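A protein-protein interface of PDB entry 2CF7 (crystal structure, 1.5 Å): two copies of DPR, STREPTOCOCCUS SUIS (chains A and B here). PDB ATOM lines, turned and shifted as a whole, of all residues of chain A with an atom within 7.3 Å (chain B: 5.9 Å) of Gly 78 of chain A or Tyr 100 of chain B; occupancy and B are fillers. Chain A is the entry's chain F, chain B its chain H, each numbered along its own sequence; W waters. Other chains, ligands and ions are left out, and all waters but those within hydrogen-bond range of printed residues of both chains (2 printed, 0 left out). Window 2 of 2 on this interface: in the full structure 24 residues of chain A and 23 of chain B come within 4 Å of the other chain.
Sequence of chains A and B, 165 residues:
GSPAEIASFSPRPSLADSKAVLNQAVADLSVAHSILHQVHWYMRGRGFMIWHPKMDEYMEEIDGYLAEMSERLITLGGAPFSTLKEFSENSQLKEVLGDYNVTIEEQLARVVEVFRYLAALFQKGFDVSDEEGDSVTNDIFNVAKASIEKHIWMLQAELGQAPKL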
ATOM      1  N   LYS A  19     -27.572 -37.534  16.901  1.00  0.00           N
ATOM      2  CA  LYS A  19     -26.739 -36.374  17.264  1.00  0.00           C
ATOM      3  C   LYS A  19     -26.496 -35.490  16.047  1.00  0.00           C
ATOM      4  O   LYS A  19     -26.589 -34.248  16.121  1.00  0.00           O
ATOM      5  CB  LYS A  19     -25.416 -36.823  17.896  1.00  0.00           C
ATOM      6  CG  LYS A  19     -25.556 -37.318  19.350  1.00  0.00           C
ATOM      7  CD  LYS A  19     -24.169 -37.538  20.013  1.00  0.00           C
ATOM      8  CE  LYS A  19     -23.396 -38.684  19.393  1.00  0.00           C
ATOM      9  NZ  LYS A  19     -22.034 -38.807  20.044  1.00  0.00           N
ATOM     10  N   ASN A  23     -27.797 -31.609  15.619  1.00  0.00           N
ATOM     11  CA  ASN A  23     -26.864 -30.485  15.434  1.00  0.00           C
ATOM     12  C   ASN A  23     -27.173 -29.748  14.135  1.00  0.00           C
ATOM     13  O   ASN A  23     -27.058 -28.515  14.062  1.00  0.00           O
ATOM     14  CB  ASN A  23     -25.397 -30.946  15.513  1.00  0.00           C
ATOM     15  CG  ASN A  23     -24.507 -29.908  16.148  1.00  0.00           C
ATOM     16  OD1 ASN A  23     -24.958 -28.932  16.745  1.00  0.00           O
ATOM     17  ND2 ASN A  23     -23.212 -30.167  16.071  1.00  0.00           N
ATOM     18  N   SER A  70     -31.131 -28.636  21.139  1.00  0.00           N
ATOM     19  CA  SER A  70     -29.787 -28.461  21.672  1.00  0.00           C
ATOM     20  C   SER A  70     -29.638 -29.192  22.999  1.00  0.00           C
ATOM     21  O   SER A  70     -28.592 -29.839  23.224  1.00  0.00           O
ATOM     22  CB  SER A  70     -29.464 -26.964  21.845  1.00  0.00           C
ATOM     23  OG  SER A  70     -30.353 -26.367  22.790  1.00  0.00           O
ATOM     24  N   ARG A  72     -31.241 -31.758  24.098  1.00  0.00           N
ATOM     25  CA  ARG A  72     -31.162 -33.201  23.862  1.00  0.00           C
ATOM     26  C   ARG A  72     -29.834 -33.652  23.304  1.00  0.00           C
ATOM     27  O   ARG A  72     -29.281 -34.683  23.756  1.00  0.00           O
ATOM     28  CB  ARG A  72     -32.279 -33.643  22.922  1.00  0.00           C
ATOM     29  CG  ARG A  72     -32.360 -35.161  22.759  1.00  0.00           C
ATOM     30  CD  ARG A  72     -32.741 -35.887  24.037  1.00  0.00           C
ATOM     31  NE  ARG A  72     -32.780 -37.332  23.757  1.00  0.00           N
ATOM     32  CZ  ARG A  72     -32.716 -38.260  24.711  1.00  0.00           C
ATOM     33  NH1 ARG A  72     -32.647 -37.909  25.992  1.00  0.00           N
ATOM     34  NH2 ARG A  72     -32.728 -39.574  24.363  1.00  0.00           N
ATOM     35  N   LEU A  73     -29.279 -32.858  22.385  1.00  0.00           N
ATOM     36  CA  LEU A  73     -27.940 -33.141  21.844  1.00  0.00           C
ATOM     37  C   LEU A  73     -26.893 -33.176  22.967  1.00  0.00           C
ATOM     38  O   LEU A  73     -26.089 -34.122  23.035  1.00  0.00           O
ATOM     39  CB  LEU A  73     -27.554 -32.089  20.808  1.00  0.00           C
ATOM     40  CG  LEU A  73     -26.144 -32.174  20.246  1.00  0.00           C
ATOM     41  CD1 LEU A  73     -25.928 -33.496  19.518  1.00  0.00           C
ATOM     42  CD2 LEU A  73     -25.940 -31.028  19.253  1.00  0.00           C
ATOM     43  N   ILE A  74     -26.924 -32.192  23.863  1.00  0.00           N
ATOM     44  CA  ILE A  74     -25.965 -32.167  24.978  1.00  0.00           C
ATOM     45  C   ILE A  74     -26.161 -33.408  25.859  1.00  0.00           C
ATOM     46  O   ILE A  74     -25.196 -34.073  26.263  1.00  0.00           O
ATOM     47  CB  ILE A  74     -26.139 -30.897  25.822  1.00  0.00           C
ATOM     48  CG1 ILE A  74     -25.839 -29.657  24.974  1.00  0.00           C
ATOM     49  CG2 ILE A  74     -25.195 -30.965  27.024  1.00  0.00           C
ATOM     50  CD1 ILE A  74     -26.384 -28.352  25.632  1.00  0.00           C
ATOM     51  N   THR A  75     -27.432 -33.694  26.170  1.00  0.00           N
ATOM     52  CA  THR A  75     -27.798 -34.830  27.004  1.00  0.00           C
ATOM     53  C   THR A  75     -27.290 -36.139  26.404  1.00  0.00           C
ATOM     54  O   THR A  75     -26.851 -37.014  27.155  1.00  0.00           O
ATOM     55  CB  THR A  75     -29.316 -34.835  27.201  1.00  0.00           C
ATOM     56  OG1 THR A  75     -29.664 -33.634  27.905  1.00  0.00           O
ATOM     57  CG2 THR A  75     -29.810 -36.038  28.009  1.00  0.00           C
ATOM     58  N   LEU A  76     -27.281 -36.235  25.077  1.00  0.00           N
ATOM     59  CA  LEU A  76     -26.793 -37.464  24.378  1.00  0.00           C
ATOM     60  C   LEU A  76     -25.272 -37.507  24.259  1.00  0.00           C
ATOM     61  O   LEU A  76     -24.719 -38.453  23.681  1.00  0.00           O
ATOM     62  CB  LEU A  76     -27.438 -37.564  22.978  1.00  0.00           C
ATOM     63  CG  LEU A  76     -28.931 -37.859  22.982  1.00  0.00           C
ATOM     64  CD1 LEU A  76     -29.471 -37.671  21.553  1.00  0.00           C
ATOM     65  CD2 LEU A  76     -29.169 -39.319  23.495  1.00  0.00           C
ATOM     66  N   GLY A  77     -24.580 -36.486  24.767  1.00  0.00           N
ATOM     67  CA  GLY A  77     -23.112 -36.501  24.690  1.00  0.00           C
ATOM     68  C   GLY A  77     -22.543 -35.795  23.489  1.00  0.00           C
ATOM     69  O   GLY A  77     -21.349 -35.902  23.202  1.00  0.00           O
ATOM     70  N   GLY A  78     -23.370 -35.017  22.817  1.00  0.00           N
ATOM     71  CA  GLY A  78     -22.891 -34.228  21.677  1.00  0.00           C
ATOM     72  C   GLY A  78     -22.453 -32.820  22.071  1.00  0.00           C
ATOM     73  O   GLY A  78     -22.409 -32.473  23.255  1.00  0.00           O
ATOM     74  N   ALA A  79     -22.113 -32.028  21.060  1.00  0.00           N
ATOM     75  CA  ALA A  79     -21.528 -30.707  21.234  1.00  0.00           C
ATOM     76  C   ALA A  79     -22.204 -29.780  20.227  1.00  0.00           C
ATOM     77  O   ALA A  79     -21.884 -29.807  19.032  1.00  0.00           O
ATOM     78  CB  ALA A  79     -20.004 -30.759  20.972  1.00  0.00           C
ATOM     79  N   PRO A  80     -23.138 -28.936  20.682  1.00  0.00           N
ATOM     80  CA  PRO A  80     -23.892 -28.125  19.705  1.00  0.00           C
ATOM     81  C   PRO A  80     -22.990 -27.088  19.032  1.00  0.00           C
ATOM     82  O   PRO A  80     -22.135 -26.473  19.670  1.00  0.00           O
ATOM     83  CB  PRO A  80     -24.941 -27.411  20.584  1.00  0.00           C
ATOM     84  CG  PRO A  80     -24.328 -27.384  21.976  1.00  0.00           C
ATOM     85  CD  PRO A  80     -23.593 -28.693  22.073  1.00  0.00           C
ATOM     86  N   TRP B  41     -24.957 -23.534  27.138  1.00  0.00           N
ATOM     87  CA  TRP B  41     -24.945 -24.936  26.707  1.00  0.00           C
ATOM     88  C   TRP B  41     -23.744 -25.717  27.267  1.00  0.00           C
ATOM     89  O   TRP B  41     -23.857 -26.900  27.639  1.00  0.00           O
ATOM     90  CB  TRP B  41     -24.860 -24.953  25.185  1.00  0.00           C
ATOM     91  CG  TRP B  41     -26.145 -24.696  24.487  1.00  0.00           C
ATOM     92  CD1 TRP B  41     -27.400 -25.016  24.926  1.00  0.00           C
ATOM     93  CD2 TRP B  41     -26.294 -24.140  23.184  1.00  0.00           C
ATOM     94  NE1 TRP B  41     -28.344 -24.647  23.974  1.00  0.00           N
ATOM     95  CE2 TRP B  41     -27.675 -24.143  22.888  1.00  0.00           C
ATOM     96  CE3 TRP B  41     -25.392 -23.641  22.233  1.00  0.00           C
ATOM     97  CZ2 TRP B  41     -28.187 -23.651  21.678  1.00  0.00           C
ATOM     98  CZ3 TRP B  41     -25.899 -23.158  21.023  1.00  0.00           C
ATOM     99  CH2 TRP B  41     -27.292 -23.185  20.750  1.00  0.00           C
ATOM    100  N   TYR B  42     -22.577 -25.071  27.249  1.00  0.00           N
ATOM    101  CA  TYR B  42     -21.334 -25.774  27.609  1.00  0.00           C
ATOM    102  C   TYR B  42     -20.955 -25.728  29.079  1.00  0.00           C
ATOM    103  O   TYR B  42     -19.975 -26.345  29.499  1.00  0.00           O
ATOM    104  CB  TYR B  42     -20.180 -25.278  26.732  1.00  0.00           C
ATOM    105  CG  TYR B  42     -20.254 -25.818  25.320  1.00  0.00           C
ATOM    106  CD1 TYR B  42     -20.992 -25.165  24.317  1.00  0.00           C
ATOM    107  CD2 TYR B  42     -19.608 -27.009  24.987  1.00  0.00           C
ATOM    108  CE1 TYR B  42     -21.087 -25.684  23.007  1.00  0.00           C
ATOM    109  CE2 TYR B  42     -19.646 -27.526  23.681  1.00  0.00           C
ATOM    110  CZ  TYR B  42     -20.400 -26.872  22.698  1.00  0.00           C
ATOM    111  OH  TYR B  42     -20.441 -27.416  21.414  1.00  0.00           O
ATOM    112  N   MET B  43     -21.747 -25.005  29.871  1.00  0.00           N
ATOM    113  CA  MET B  43     -21.423 -24.784  31.280  1.00  0.00           C
ATOM    114  C   MET B  43     -21.313 -26.073  32.065  1.00  0.00           C
ATOM    115  O   MET B  43     -22.148 -26.960  31.950  1.00  0.00           O
ATOM    116  CB  MET B  43     -22.552 -23.939  31.888  1.00  0.00           C
ATOM    117  CG  MET B  43     -22.191 -23.438  33.263  1.00  0.00           C
ATOM    118  SD  MET B  43     -23.486 -22.386  33.962  1.00  0.00           S
ATOM    119  CE  MET B  43     -23.315 -20.958  32.901  1.00  0.00           C
ATOM    120  N   ARG B  44     -20.226 -26.137  32.836  1.00  0.00           N
ATOM    121  CA  ARG B  44     -20.036 -27.202  33.839  1.00  0.00           C
ATOM    122  C   ARG B  44     -19.355 -26.640  35.069  1.00  0.00           C
ATOM    123  O   ARG B  44     -18.512 -25.741  34.964  1.00  0.00           O
ATOM    124  CB  ARG B  44     -19.190 -28.343  33.297  1.00  0.00           C
ATOM    125  CG  ARG B  44     -19.841 -29.071  32.134  1.00  0.00           C
ATOM    126  CD  ARG B  44     -19.071 -30.316  31.967  1.00  0.00           C
ATOM    127  NE  ARG B  44     -19.507 -31.112  30.845  1.00  0.00           N
ATOM    128  CZ  ARG B  44     -18.702 -32.032  30.300  1.00  0.00           C
ATOM    129  NH1 ARG B  44     -17.479 -32.216  30.794  1.00  0.00           N
ATOM    130  NH2 ARG B  44     -19.126 -32.735  29.278  1.00  0.00           N
ATOM    131  N   GLY B  98     -17.100 -24.057  21.092  1.00  0.00           N
ATOM    132  CA  GLY B  98     -17.584 -24.459  22.430  1.00  0.00           C
ATOM    133  C   GLY B  98     -16.694 -25.537  23.020  1.00  0.00           C
ATOM    134  O   GLY B  98     -16.222 -26.417  22.300  1.00  0.00           O
ATOM    135  N   ASP B  99     -16.517 -25.499  24.337  1.00  0.00           N
ATOM    136  CA  ASP B  99     -15.632 -26.444  25.042  1.00  0.00           C
ATOM    137  C   ASP B  99     -16.231 -26.666  26.431  1.00  0.00           C
ATOM    138  O   ASP B  99     -16.329 -25.745  27.243  1.00  0.00           O
ATOM    139  CB  ASP B  99     -14.236 -25.804  25.169  1.00  0.00           C
ATOM    140  CG  ASP B  99     -13.228 -26.685  25.857  1.00  0.00           C
ATOM    141  OD1 ASP B  99     -13.539 -27.819  26.262  1.00  0.00           O
ATOM    142  OD2 ASP B  99     -12.069 -26.224  25.935  1.00  0.00           O
ATOM    143  N   TYR B 100     -16.581 -27.916  26.723  1.00  0.00           N
ATOM    144  CA  TYR B 100     -17.128 -28.226  28.055  1.00  0.00           C
ATOM    145  C   TYR B 100     -16.136 -28.130  29.194  1.00  0.00           C
ATOM    146  O   TYR B 100     -16.536 -28.069  30.354  1.00  0.00           O
ATOM    147  CB  TYR B 100     -17.683 -29.658  28.105  1.00  0.00           C
ATOM    148  CG  TYR B 100     -18.937 -29.847  27.262  1.00  0.00           C
ATOM    149  CD1 TYR B 100     -18.885 -30.576  26.073  1.00  0.00           C
ATOM    150  CD2 TYR B 100     -20.174 -29.292  27.646  1.00  0.00           C
ATOM    151  CE1 TYR B 100     -20.042 -30.741  25.286  1.00  0.00           C
ATOM    152  CE2 TYR B 100     -21.306 -29.430  26.868  1.00  0.00           C
ATOM    153  CZ  TYR B 100     -21.243 -30.162  25.677  1.00  0.00           C
ATOM    154  OH  TYR B 100     -22.377 -30.327  24.932  1.00  0.00           O
ATOM    155  N   ASN B 101     -14.855 -28.144  28.846  1.00  0.00           N
ATOM    156  CA  ASN B 101     -13.846 -28.135  29.913  1.00  0.00           C
ATOM    157  C   ASN B 101     -13.488 -26.776  30.487  1.00  0.00           C
ATOM    158  O   ASN B 101     -12.719 -26.678  31.435  1.00  0.00           O
ATOM    159  CB  ASN B 101     -12.672 -29.000  29.536  1.00  0.00           C
ATOM    160  CG  ASN B 101     -13.078 -30.476  29.391  1.00  0.00           C
ATOM    161  OD1 ASN B 101     -13.710 -31.071  30.281  1.00  0.00           O
ATOM    162  ND2 ASN B 101     -12.743 -31.052  28.242  1.00  0.00           N
ATOM    163  N   VAL B 102     -14.094 -25.734  29.968  1.00  0.00           N
ATOM    164  CA  VAL B 102     -13.992 -24.421  30.562  1.00  0.00           C
ATOM    165  C   VAL B 102     -14.653 -24.472  31.938  1.00  0.00           C
ATOM    166  O   VAL B 102     -15.715 -25.107  32.105  1.00  0.00           O
ATOM    167  CB  VAL B 102     -14.641 -23.406  29.612  1.00  0.00           C
ATOM    168  CG1 VAL B 102     -14.562 -21.987  30.184  1.00  0.00           C
ATOM    169  CG2 VAL B 102     -13.950 -23.440  28.227  1.00  0.00           C
ATOM    170  N   THR B 103     -14.028 -23.866  32.945  1.00  0.00           N
ATOM    171  CA  THR B 103     -14.605 -23.898  34.295  1.00  0.00           C
ATOM    172  C   THR B 103     -15.670 -22.848  34.471  1.00  0.00           C
ATOM    173  O   THR B 103     -15.766 -21.889  33.684  1.00  0.00           O
ATOM    174  CB  THR B 103     -13.556 -23.689  35.377  1.00  0.00           C
ATOM    175  OG1 THR B 103     -12.928 -22.398  35.239  1.00  0.00           O
ATOM    176  CG2 THR B 103     -12.514 -24.846  35.297  1.00  0.00           C
HETATM  177  O   HOH W   1     -31.460 -23.275  23.896  1.00  0.00           O
HETATM  178  O   HOH W   2     -22.489 -33.601  25.907  1.00  0.00           O
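No position is printed for both chains.
Of the 9 pairs that touch across the chains among the printed residues, none has its exchanged pair printed and touching as well.
The backbone carbonyl oxygen (O) of Ala 79 of chain A sits at hydrogen-bond distance from the side-chain amide nitrogen (ND2) of Asn 23 of chain A, 3.3 Å away.
The backbone carbonyl oxygen of Leu 73 of chain A sits at hydrogen-bond distance from the backbone NH of Gly 78 of chain A.
Hydrophobic or aromatic side chains of chain A that line the printed part of chain B: Ile 74, Ala 79 and Pro 80.
Along chain A the printed residues that touch a printed residue of chain B span positions 70 to 80.
Among the printed residues, no Asp or Glu carboxylate lies within 4 Å of a Lys or Arg side-chain nitrogen of the other chain.
Among the printed residues, pairs that only touch across the chains: Ala 79 of chain A with Tyr 42 of chain B (3.2 Å), Pro 80 of chain A with Tyr 100 of chain B (3.5 Å), Ile 74 of chain A with Tyr 100 of chain B (3.5 Å), Ile 74 of chain A with Trp 41 of chain B (3.5 Å), Ala 79 of chain A with Tyr 100 of chain B (3.8 Å) and Pro 80 of chain A with Trp 41 of chain B (3.9 Å).
Gly 78 of chain A touches one residue of chain B.
Of chain A, only Ile 74, Gly 78, Ala 79 and Pro 80 come within 4 Å of Tyr 100 of chain B.
Of the printed residues of chain B, Ile 74 of chain A touches Trp 41 (3.5 Å) and Tyr 100 (3.5 Å).
Printed residues of chain B within 4 Å of Ala 79 of chain A: Tyr 42 and Tyr 100.
Of the printed residues of chain B, Pro 80 of chain A touches Trp 41, Tyr 42 and Tyr 100.
Printed residues of chain B within 4 Å of Ser 70 of chain A: Trp 41 (2.9 Å).
Gly 98 of chain B touches none of the printed residues of chain A.
The nearest printed residue of chain A that does not touch Tyr 100 of chain B is Leu 73 of chain A (5.6 Å).
Water W2 lies within hydrogen-bond range of O of Ile 74 of chain A (2.8 Å), O of Gly 78 of chain A (2.9 Å) and OH of Tyr 100 of chain B (3.4 Å).
Water W1 lies within hydrogen-bond range of NE1 of Trp 41 of chain B (3.4 Å) and OG of Ser 70 of chain A (3.5 Å).
The backbone carbonyl oxygen (O) of Pro 80 of chain A lies within hydrogen-bond range of the side-chain hydroxyl (OH) of Tyr 42 of chain B (2.6 Å).
The side-chain hydroxyl of Ser 70 of chain A sits at hydrogen-bond distance from the indole nitrogen of Trp 41 of chain B (2.9 Å).
The backbone carbonyl oxygen (O) of Gly 78 of chain A lies within hydrogen-bond range of the side-chain hydroxyl (OH) of Tyr 100 of chain B.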
